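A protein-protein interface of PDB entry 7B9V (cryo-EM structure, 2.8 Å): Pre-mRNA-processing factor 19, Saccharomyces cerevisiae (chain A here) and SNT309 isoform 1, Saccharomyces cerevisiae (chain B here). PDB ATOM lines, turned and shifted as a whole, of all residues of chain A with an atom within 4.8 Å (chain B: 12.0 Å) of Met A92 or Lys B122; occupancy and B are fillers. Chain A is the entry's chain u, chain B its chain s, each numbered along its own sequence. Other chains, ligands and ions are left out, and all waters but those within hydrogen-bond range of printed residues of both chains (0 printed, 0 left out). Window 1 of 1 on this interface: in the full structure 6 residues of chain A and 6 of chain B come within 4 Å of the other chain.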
ATOM      1  N   TRP A  88      23.582  22.151 -29.922  1.00  0.00           N
ATOM      2  CA  TRP A  88      23.960  20.742 -29.891  1.00  0.00           C
ATOM      3  C   TRP A  88      23.035  20.006 -28.926  1.00  0.00           C
ATOM      4  O   TRP A  88      22.562  18.912 -29.227  1.00  0.00           O
ATOM      5  CB  TRP A  88      25.454  20.540 -29.573  1.00  0.00           C
ATOM      6  CG  TRP A  88      25.892  19.069 -29.838  1.00  0.00           C
ATOM      7  CD1 TRP A  88      25.450  17.932 -29.219  1.00  0.00           C
ATOM      8  CD2 TRP A  88      26.774  18.625 -30.887  1.00  0.00           C
ATOM      9  NE1 TRP A  88      26.000  16.840 -29.790  1.00  0.00           N
ATOM     10  CE2 TRP A  88      26.818  17.221 -30.808  1.00  0.00           C
ATOM     11  CE3 TRP A  88      27.543  19.270 -31.844  1.00  0.00           C
ATOM     12  CZ2 TRP A  88      27.598  16.455 -31.665  1.00  0.00           C
ATOM     13  CZ3 TRP A  88      28.320  18.508 -32.693  1.00  0.00           C
ATOM     14  CH2 TRP A  88      28.343  17.111 -32.592  1.00  0.00           C
ATOM     15  N   ASP A  89      22.822  20.553 -27.734  1.00  0.00           N
ATOM     16  CA  ASP A  89      21.822  20.017 -26.808  1.00  0.00           C
ATOM     17  C   ASP A  89      20.404  20.085 -27.390  1.00  0.00           C
ATOM     18  O   ASP A  89      19.550  19.314 -26.966  1.00  0.00           O
ATOM     19  CB  ASP A  89      21.880  20.718 -25.443  1.00  0.00           C
ATOM     20  CG  ASP A  89      23.127  20.353 -24.650  1.00  0.00           C
ATOM     21  OD1 ASP A  89      23.615  19.213 -24.797  1.00  0.00           O
ATOM     22  OD2 ASP A  89      23.595  21.190 -23.853  1.00  0.00           O
ATOM     23  N   ALA A  90      20.133  20.988 -28.328  1.00  0.00           N
ATOM     24  CA  ALA A  90      18.895  20.915 -29.108  1.00  0.00           C
ATOM     25  C   ALA A  90      18.864  19.712 -30.062  1.00  0.00           C
ATOM     26  O   ALA A  90      17.795  19.086 -30.192  1.00  0.00           O
ATOM     27  CB  ALA A  90      18.671  22.223 -29.870  1.00  0.00           C
ATOM     28  N   ILE A  91      19.985  19.387 -30.762  1.00  0.00           N
ATOM     29  CA  ILE A  91      20.093  18.057 -31.425  1.00  0.00           C
ATOM     30  C   ILE A  91      19.820  16.938 -30.434  1.00  0.00           C
ATOM     31  O   ILE A  91      19.121  15.974 -30.731  1.00  0.00           O
ATOM     32  CB  ILE A  91      21.476  17.754 -32.055  1.00  0.00           C
ATOM     33  CG1 ILE A  91      22.217  18.812 -32.824  1.00  0.00           C
ATOM     34  CG2 ILE A  91      21.431  16.508 -32.927  1.00  0.00           C
ATOM     35  CD1 ILE A  91      23.727  18.407 -32.753  1.00  0.00           C
ATOM     36  N   MET A  92      20.431  17.026 -29.281  1.00  0.00           N
ATOM     37  CA  MET A  92      20.568  15.905 -28.373  1.00  0.00           C
ATOM     38  C   MET A  92      19.287  15.691 -27.553  1.00  0.00           C
ATOM     39  O   MET A  92      18.948  14.557 -27.209  1.00  0.00           O
ATOM     40  CB  MET A  92      21.796  16.143 -27.529  1.00  0.00           C
ATOM     41  CG  MET A  92      22.307  14.938 -26.914  1.00  0.00           C
ATOM     42  SD  MET A  92      22.873  13.635 -28.015  1.00  0.00           S
ATOM     43  CE  MET A  92      23.933  14.394 -29.153  1.00  0.00           C
ATOM     44  N   LEU A  93      18.560  16.769 -27.257  1.00  0.00           N
ATOM     45  CA  LEU A  93      17.171  16.686 -26.809  1.00  0.00           C
ATOM     46  C   LEU A  93      16.300  16.116 -27.916  1.00  0.00           C
ATOM     47  O   LEU A  93      15.390  15.331 -27.647  1.00  0.00           O
ATOM     48  CB  LEU A  93      16.639  18.038 -26.321  1.00  0.00           C
ATOM     49  CG  LEU A  93      15.179  18.155 -25.808  1.00  0.00           C
ATOM     50  CD1 LEU A  93      15.146  19.238 -24.778  1.00  0.00           C
ATOM     51  CD2 LEU A  93      14.119  18.562 -26.855  1.00  0.00           C
ATOM     52  N   GLU A  94      16.480  16.599 -29.146  1.00  0.00           N
ATOM     53  CA  GLU A  94      15.755  16.069 -30.302  1.00  0.00           C
ATOM     54  C   GLU A  94      16.012  14.567 -30.503  1.00  0.00           C
ATOM     55  O   GLU A  94      15.089  13.808 -30.816  1.00  0.00           O
ATOM     56  CB  GLU A  94      16.075  16.903 -31.544  1.00  0.00           C
ATOM     57  CG  GLU A  94      15.173  16.601 -32.676  1.00  0.00           C
ATOM     58  N   ASN A  95      17.256  14.137 -30.360  1.00  0.00           N
ATOM     59  CA  ASN A  95      17.657  12.730 -30.439  1.00  0.00           C
ATOM     60  C   ASN A  95      16.998  11.957 -29.284  1.00  0.00           C
ATOM     61  O   ASN A  95      16.602  10.800 -29.480  1.00  0.00           O
ATOM     62  CB  ASN A  95      19.191  12.492 -30.552  1.00  0.00           C
ATOM     63  CG  ASN A  95      19.911  12.507 -29.252  1.00  0.00           C
ATOM     64  N   PHE A  96      16.965  12.522 -28.052  1.00  0.00           N
ATOM     65  CA  PHE A  96      16.199  11.861 -26.977  1.00  0.00           C
ATOM     66  C   PHE A  96      14.723  11.732 -27.306  1.00  0.00           C
ATOM     67  O   PHE A  96      14.135  10.694 -26.999  1.00  0.00           O
ATOM     68  CB  PHE A  96      16.300  12.613 -25.606  1.00  0.00           C
ATOM     69  CG  PHE A  96      15.013  12.649 -24.766  1.00  0.00           C
ATOM     70  CD1 PHE A  96      14.707  11.557 -23.953  1.00  0.00           C
ATOM     71  CD2 PHE A  96      14.190  13.783 -24.723  1.00  0.00           C
ATOM     72  CE1 PHE A  96      13.544  11.560 -23.201  1.00  0.00           C
ATOM     73  CE2 PHE A  96      13.019  13.774 -23.962  1.00  0.00           C
ATOM     74  CZ  PHE A  96      12.710  12.663 -23.201  1.00  0.00           C
ATOM     75  N   LEU B 114      15.705  18.545 -15.857  1.00  0.00           N
ATOM     76  CA  LEU B 114      15.226  17.452 -16.700  1.00  0.00           C
ATOM     77  C   LEU B 114      15.903  17.434 -18.080  1.00  0.00           C
ATOM     78  O   LEU B 114      16.539  16.445 -18.426  1.00  0.00           O
ATOM     79  CB  LEU B 114      13.708  17.498 -16.858  1.00  0.00           C
ATOM     80  CG  LEU B 114      13.185  16.283 -17.631  1.00  0.00           C
ATOM     81  N   GLY B 115      15.744  18.510 -18.869  1.00  0.00           N
ATOM     82  CA  GLY B 115      16.139  18.511 -20.281  1.00  0.00           C
ATOM     83  C   GLY B 115      17.631  18.388 -20.539  1.00  0.00           C
ATOM     84  O   GLY B 115      18.045  17.801 -21.554  1.00  0.00           O
ATOM     85  N   ILE B 116      18.449  18.913 -19.619  1.00  0.00           N
ATOM     86  CA  ILE B 116      19.888  18.644 -19.613  1.00  0.00           C
ATOM     87  C   ILE B 116      20.148  17.148 -19.464  1.00  0.00           C
ATOM     88  O   ILE B 116      20.858  16.562 -20.278  1.00  0.00           O
ATOM     89  CB  ILE B 116      20.620  19.479 -18.540  1.00  0.00           C
ATOM     90  CG1 ILE B 116      20.425  20.979 -18.806  1.00  0.00           C
ATOM     91  CG2 ILE B 116      22.112  19.120 -18.506  1.00  0.00           C
ATOM     92  CD1 ILE B 116      21.287  21.900 -17.943  1.00  0.00           C
ATOM     93  N   VAL B 117      19.501  16.504 -18.489  1.00  0.00           N
ATOM     94  CA  VAL B 117      19.596  15.051 -18.270  1.00  0.00           C
ATOM     95  C   VAL B 117      19.043  14.249 -19.462  1.00  0.00           C
ATOM     96  O   VAL B 117      19.577  13.186 -19.786  1.00  0.00           O
ATOM     97  CB  VAL B 117      18.927  14.683 -16.922  1.00  0.00           C
ATOM     98  CG1 VAL B 117      19.014  13.195 -16.610  1.00  0.00           C
ATOM     99  CG2 VAL B 117      19.619  15.438 -15.797  1.00  0.00           C
ATOM    100  N   ASP B 118      17.964  14.716 -20.102  1.00  0.00           N
ATOM    101  CA  ASP B 118      17.448  14.102 -21.345  1.00  0.00           C
ATOM    102  C   ASP B 118      18.515  14.032 -22.446  1.00  0.00           C
ATOM    103  O   ASP B 118      18.865  12.930 -22.939  1.00  0.00           O
ATOM    104  CB  ASP B 118      16.235  14.883 -21.865  1.00  0.00           C
ATOM    105  CG  ASP B 118      14.987  14.646 -21.043  1.00  0.00           C
ATOM    106  N   SER B 119      19.114  15.184 -22.769  1.00  0.00           N
ATOM    107  CA  SER B 119      20.211  15.196 -23.740  1.00  0.00           C
ATOM    108  C   SER B 119      21.449  14.442 -23.235  1.00  0.00           C
ATOM    109  O   SER B 119      22.075  13.711 -24.002  1.00  0.00           O
ATOM    110  CB  SER B 119      20.568  16.645 -24.071  1.00  0.00           C
ATOM    111  N   TYR B 120      21.791  14.544 -21.952  1.00  0.00           N
ATOM    112  CA  TYR B 120      22.953  13.830 -21.405  1.00  0.00           C
ATOM    113  C   TYR B 120      22.778  12.307 -21.389  1.00  0.00           C
ATOM    114  O   TYR B 120      23.769  11.597 -21.539  1.00  0.00           O
ATOM    115  CB  TYR B 120      23.376  14.382 -20.046  1.00  0.00           C
ATOM    116  CG  TYR B 120      23.786  15.839 -20.099  1.00  0.00           C
ATOM    117  N   LEU B 121      21.560  11.788 -21.172  1.00  0.00           N
ATOM    118  CA  LEU B 121      21.296  10.346 -21.323  1.00  0.00           C
ATOM    119  C   LEU B 121      21.525   9.878 -22.761  1.00  0.00           C
ATOM    120  O   LEU B 121      22.035   8.766 -22.989  1.00  0.00           O
ATOM    121  CB  LEU B 121      19.868  10.015 -20.874  1.00  0.00           C
ATOM    122  CG  LEU B 121      19.607   9.931 -19.370  1.00  0.00           C
ATOM    123  CD1 LEU B 121      18.116  10.049 -19.081  1.00  0.00           C
ATOM    124  CD2 LEU B 121      20.176   8.651 -18.798  1.00  0.00           C
ATOM    125  N   LYS B 122      21.171  10.719 -23.740  1.00  0.00           N
ATOM    126  CA  LYS B 122      21.544  10.441 -25.142  1.00  0.00           C
ATOM    127  C   LYS B 122      23.051  10.462 -25.344  1.00  0.00           C
ATOM    128  O   LYS B 122      23.577   9.694 -26.168  1.00  0.00           O
ATOM    129  CB  LYS B 122      20.905  11.416 -26.071  1.00  0.00           C
ATOM    130  CG  LYS B 122      19.603  11.444 -25.832  1.00  0.00           C
ATOM    131  N   HIS B 123      23.710  11.484 -24.771  1.00  0.00           N
ATOM    132  CA  HIS B 123      25.176  11.551 -24.752  1.00  0.00           C
ATOM    133  C   HIS B 123      25.752  10.248 -24.238  1.00  0.00           C
ATOM    134  O   HIS B 123      26.519   9.635 -24.954  1.00  0.00           O
ATOM    135  CB  HIS B 123      25.792  12.718 -23.952  1.00  0.00           C
ATOM    136  CG  HIS B 123      25.482  14.112 -24.429  1.00  0.00           C
ATOM    137  ND1 HIS B 123      25.008  15.093 -23.575  1.00  0.00           N
ATOM    138  CD2 HIS B 123      25.413  14.640 -25.678  1.00  0.00           C
ATOM    139  CE1 HIS B 123      24.708  16.166 -24.277  1.00  0.00           C
ATOM    140  NE2 HIS B 123      24.988  15.935 -25.550  1.00  0.00           N
ATOM    141  N   GLN B 124      25.300   9.765 -23.072  1.00  0.00           N
ATOM    142  CA  GLN B 124      25.687   8.465 -22.487  1.00  0.00           C
ATOM    143  C   GLN B 124      25.511   7.308 -23.478  1.00  0.00           C
ATOM    144  O   GLN B 124      26.432   6.513 -23.670  1.00  0.00           O
ATOM    145  CB  GLN B 124      24.995   8.200 -21.153  1.00  0.00           C
ATOM    146  CG  GLN B 124      25.382   9.231 -20.092  1.00  0.00           C
ATOM    147  CD  GLN B 124      25.418   8.698 -18.667  1.00  0.00           C
ATOM    148  OE1 GLN B 124      25.028   7.571 -18.408  1.00  0.00           O
ATOM    149  NE2 GLN B 124      25.906   9.522 -17.753  1.00  0.00           N
ATOM    150  N   GLU B 125      24.371   7.256 -24.165  1.00  0.00           N
ATOM    151  CA  GLU B 125      24.102   6.295 -25.251  1.00  0.00           C
ATOM    152  C   GLU B 125      25.073   6.446 -26.447  1.00  0.00           C
ATOM    153  O   GLU B 125      25.351   5.451 -27.130  1.00  0.00           O
ATOM    154  CB  GLU B 125      22.662   6.415 -25.713  1.00  0.00           C
ATOM    155  N   ILE B 126      25.638   7.642 -26.688  1.00  0.00           N
ATOM    156  CA  ILE B 126      26.740   7.751 -27.673  1.00  0.00           C
ATOM    157  C   ILE B 126      28.007   7.146 -27.069  1.00  0.00           C
ATOM    158  O   ILE B 126      28.711   6.374 -27.747  1.00  0.00           O
ATOM    159  CB  ILE B 126      27.085   9.223 -28.046  1.00  0.00           C
ATOM    160  CG1 ILE B 126      25.956  10.112 -28.537  1.00  0.00           C
ATOM    161  CG2 ILE B 126      28.381   9.370 -28.931  1.00  0.00           C
ATOM    162  CD1 ILE B 126      26.439  11.584 -28.421  1.00  0.00           C
ATOM    163  N   VAL B 127      28.324   7.510 -25.805  1.00  0.00           N
ATOM    164  CA  VAL B 127      29.563   7.081 -25.126  1.00  0.00           C
ATOM    165  C   VAL B 127      29.646   5.568 -25.044  1.00  0.00           C
ATOM    166  O   VAL B 127      30.744   4.998 -25.109  1.00  0.00           O
ATOM    167  CB  VAL B 127      29.634   7.607 -23.671  1.00  0.00           C
ATOM    168  CG1 VAL B 127      31.045   7.582 -23.116  1.00  0.00           C
ATOM    169  CG2 VAL B 127      29.200   8.937 -23.524  1.00  0.00           C
ATOM    170  N   LEU B 128      28.497   4.919 -24.818  1.00  0.00           N
ATOM    171  CA  LEU B 128      28.368   3.464 -24.859  1.00  0.00           C
ATOM    172  C   LEU B 128      28.893   2.876 -26.165  1.00  0.00           C
ATOM    173  O   LEU B 128      29.699   1.938 -26.133  1.00  0.00           O
ATOM    174  CB  LEU B 128      26.927   3.021 -24.599  1.00  0.00           C
ATOM    175  CG  LEU B 128      26.229   3.306 -23.267  1.00  0.00           C
ATOM    176  N   ASP B 129      28.337   3.335 -27.311  1.00  0.00           N
ATOM    177  CA  ASP B 129      28.721   2.839 -28.640  1.00  0.00           C
ATOM    178  C   ASP B 129      30.225   2.938 -28.881  1.00  0.00           C
ATOM    179  O   ASP B 129      30.829   2.039 -29.478  1.00  0.00           O
ATOM    180  CB  ASP B 129      28.009   3.654 -29.721  1.00  0.00           C
ATOM    181  CG  ASP B 129      26.511   3.484 -29.699  1.00  0.00           C
ATOM    182  N   THR B 130      30.830   4.025 -28.422  1.00  0.00           N
ATOM    183  CA  THR B 130      32.191   4.393 -28.774  1.00  0.00           C
ATOM    184  C   THR B 130      33.199   3.496 -28.042  1.00  0.00           C
ATOM    185  O   THR B 130      33.705   2.522 -28.589  1.00  0.00           O
ATOM    186  CB  THR B 130      32.450   5.837 -28.468  1.00  0.00           C
ATOM    187  OG1 THR B 130      31.501   6.651 -29.169  1.00  0.00           O
ATOM    188  CG2 THR B 130      33.827   6.232 -28.930  1.00  0.00           C
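Met A92 touches just these residues of chain B: Ser B119 (3.2 Å), Lys B122 (3.5 Å), His B123 (3.2 Å) and Ile B126 (3.8 Å). Of chain A, only Met A92, Asn A95 and Phe A96 come within 4 Å of Lys B122. No residue of chain B comes within 4 Å of Trp A88. Asp A89 touches one residue of chain B. Ala A90 touches none of the printed residues of chain B. No residue of chain B comes within 4 Å of Ile A91. Leu A93 touches just one residue of chain B: Ser B119 (3.8 Å). Of the printed residues of chain A, Asp B118 touches Phe A96. Of the printed residues of chain A, Ile B126 touches Met A92. Ile B116 touches none of the printed residues of chain A. Thr B130 touches none of the printed residues of chain A. The nearest residue of chain B that does not touch Met A92 is Asp B118 (4.6 Å).
ND1 of His B123 sits at hydrogen-bond distance from O of Ser B119, at 3.3 Å. The side-chain hydroxyl of Thr B130 sits at hydrogen-bond distance from the backbone carbonyl oxygen of Ile B126 (3.1 Å).
Printed residues of chain B that touch a printed residue of chain A: Asp B118, Ser B119, Lys B122, His B123 and Ile B126. Of the 9 printed residues of chain A, 5 touch a printed residue of chain B. Hydrophobic or aromatic side chains of chain A within 4 Å of the printed part of chain B: Met A92 and Phe A96. Among the printed residues, 9 pairs touch across the chains. Among the printed residues, no Asp or Glu carboxylate lies within 4 Å of a Lys or Arg side-chain nitrogen of the other chain.
OD1 of Asp A89 touches CE1 of His B123, 3.3 Å away. Met A92 touches Ser B119. CG of Lys B122 touches O of Met A92 (3.5 Å). CG of Met A92 touches NE2 of His B123, at 3.2 Å. CD1 of Ile B126 touches CE of Met A92, 3.8 Å away. N of Leu A93 touches CB of Ser B119, at 3.8 Å. CG of Asn A95 touches CB of Lys B122, 3.5 Å away. CE2 of Phe A96 touches CG of Asp B118 (3.6 Å). CB of Phe A96 touches CG of Lys B122, 3.5 Å away.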
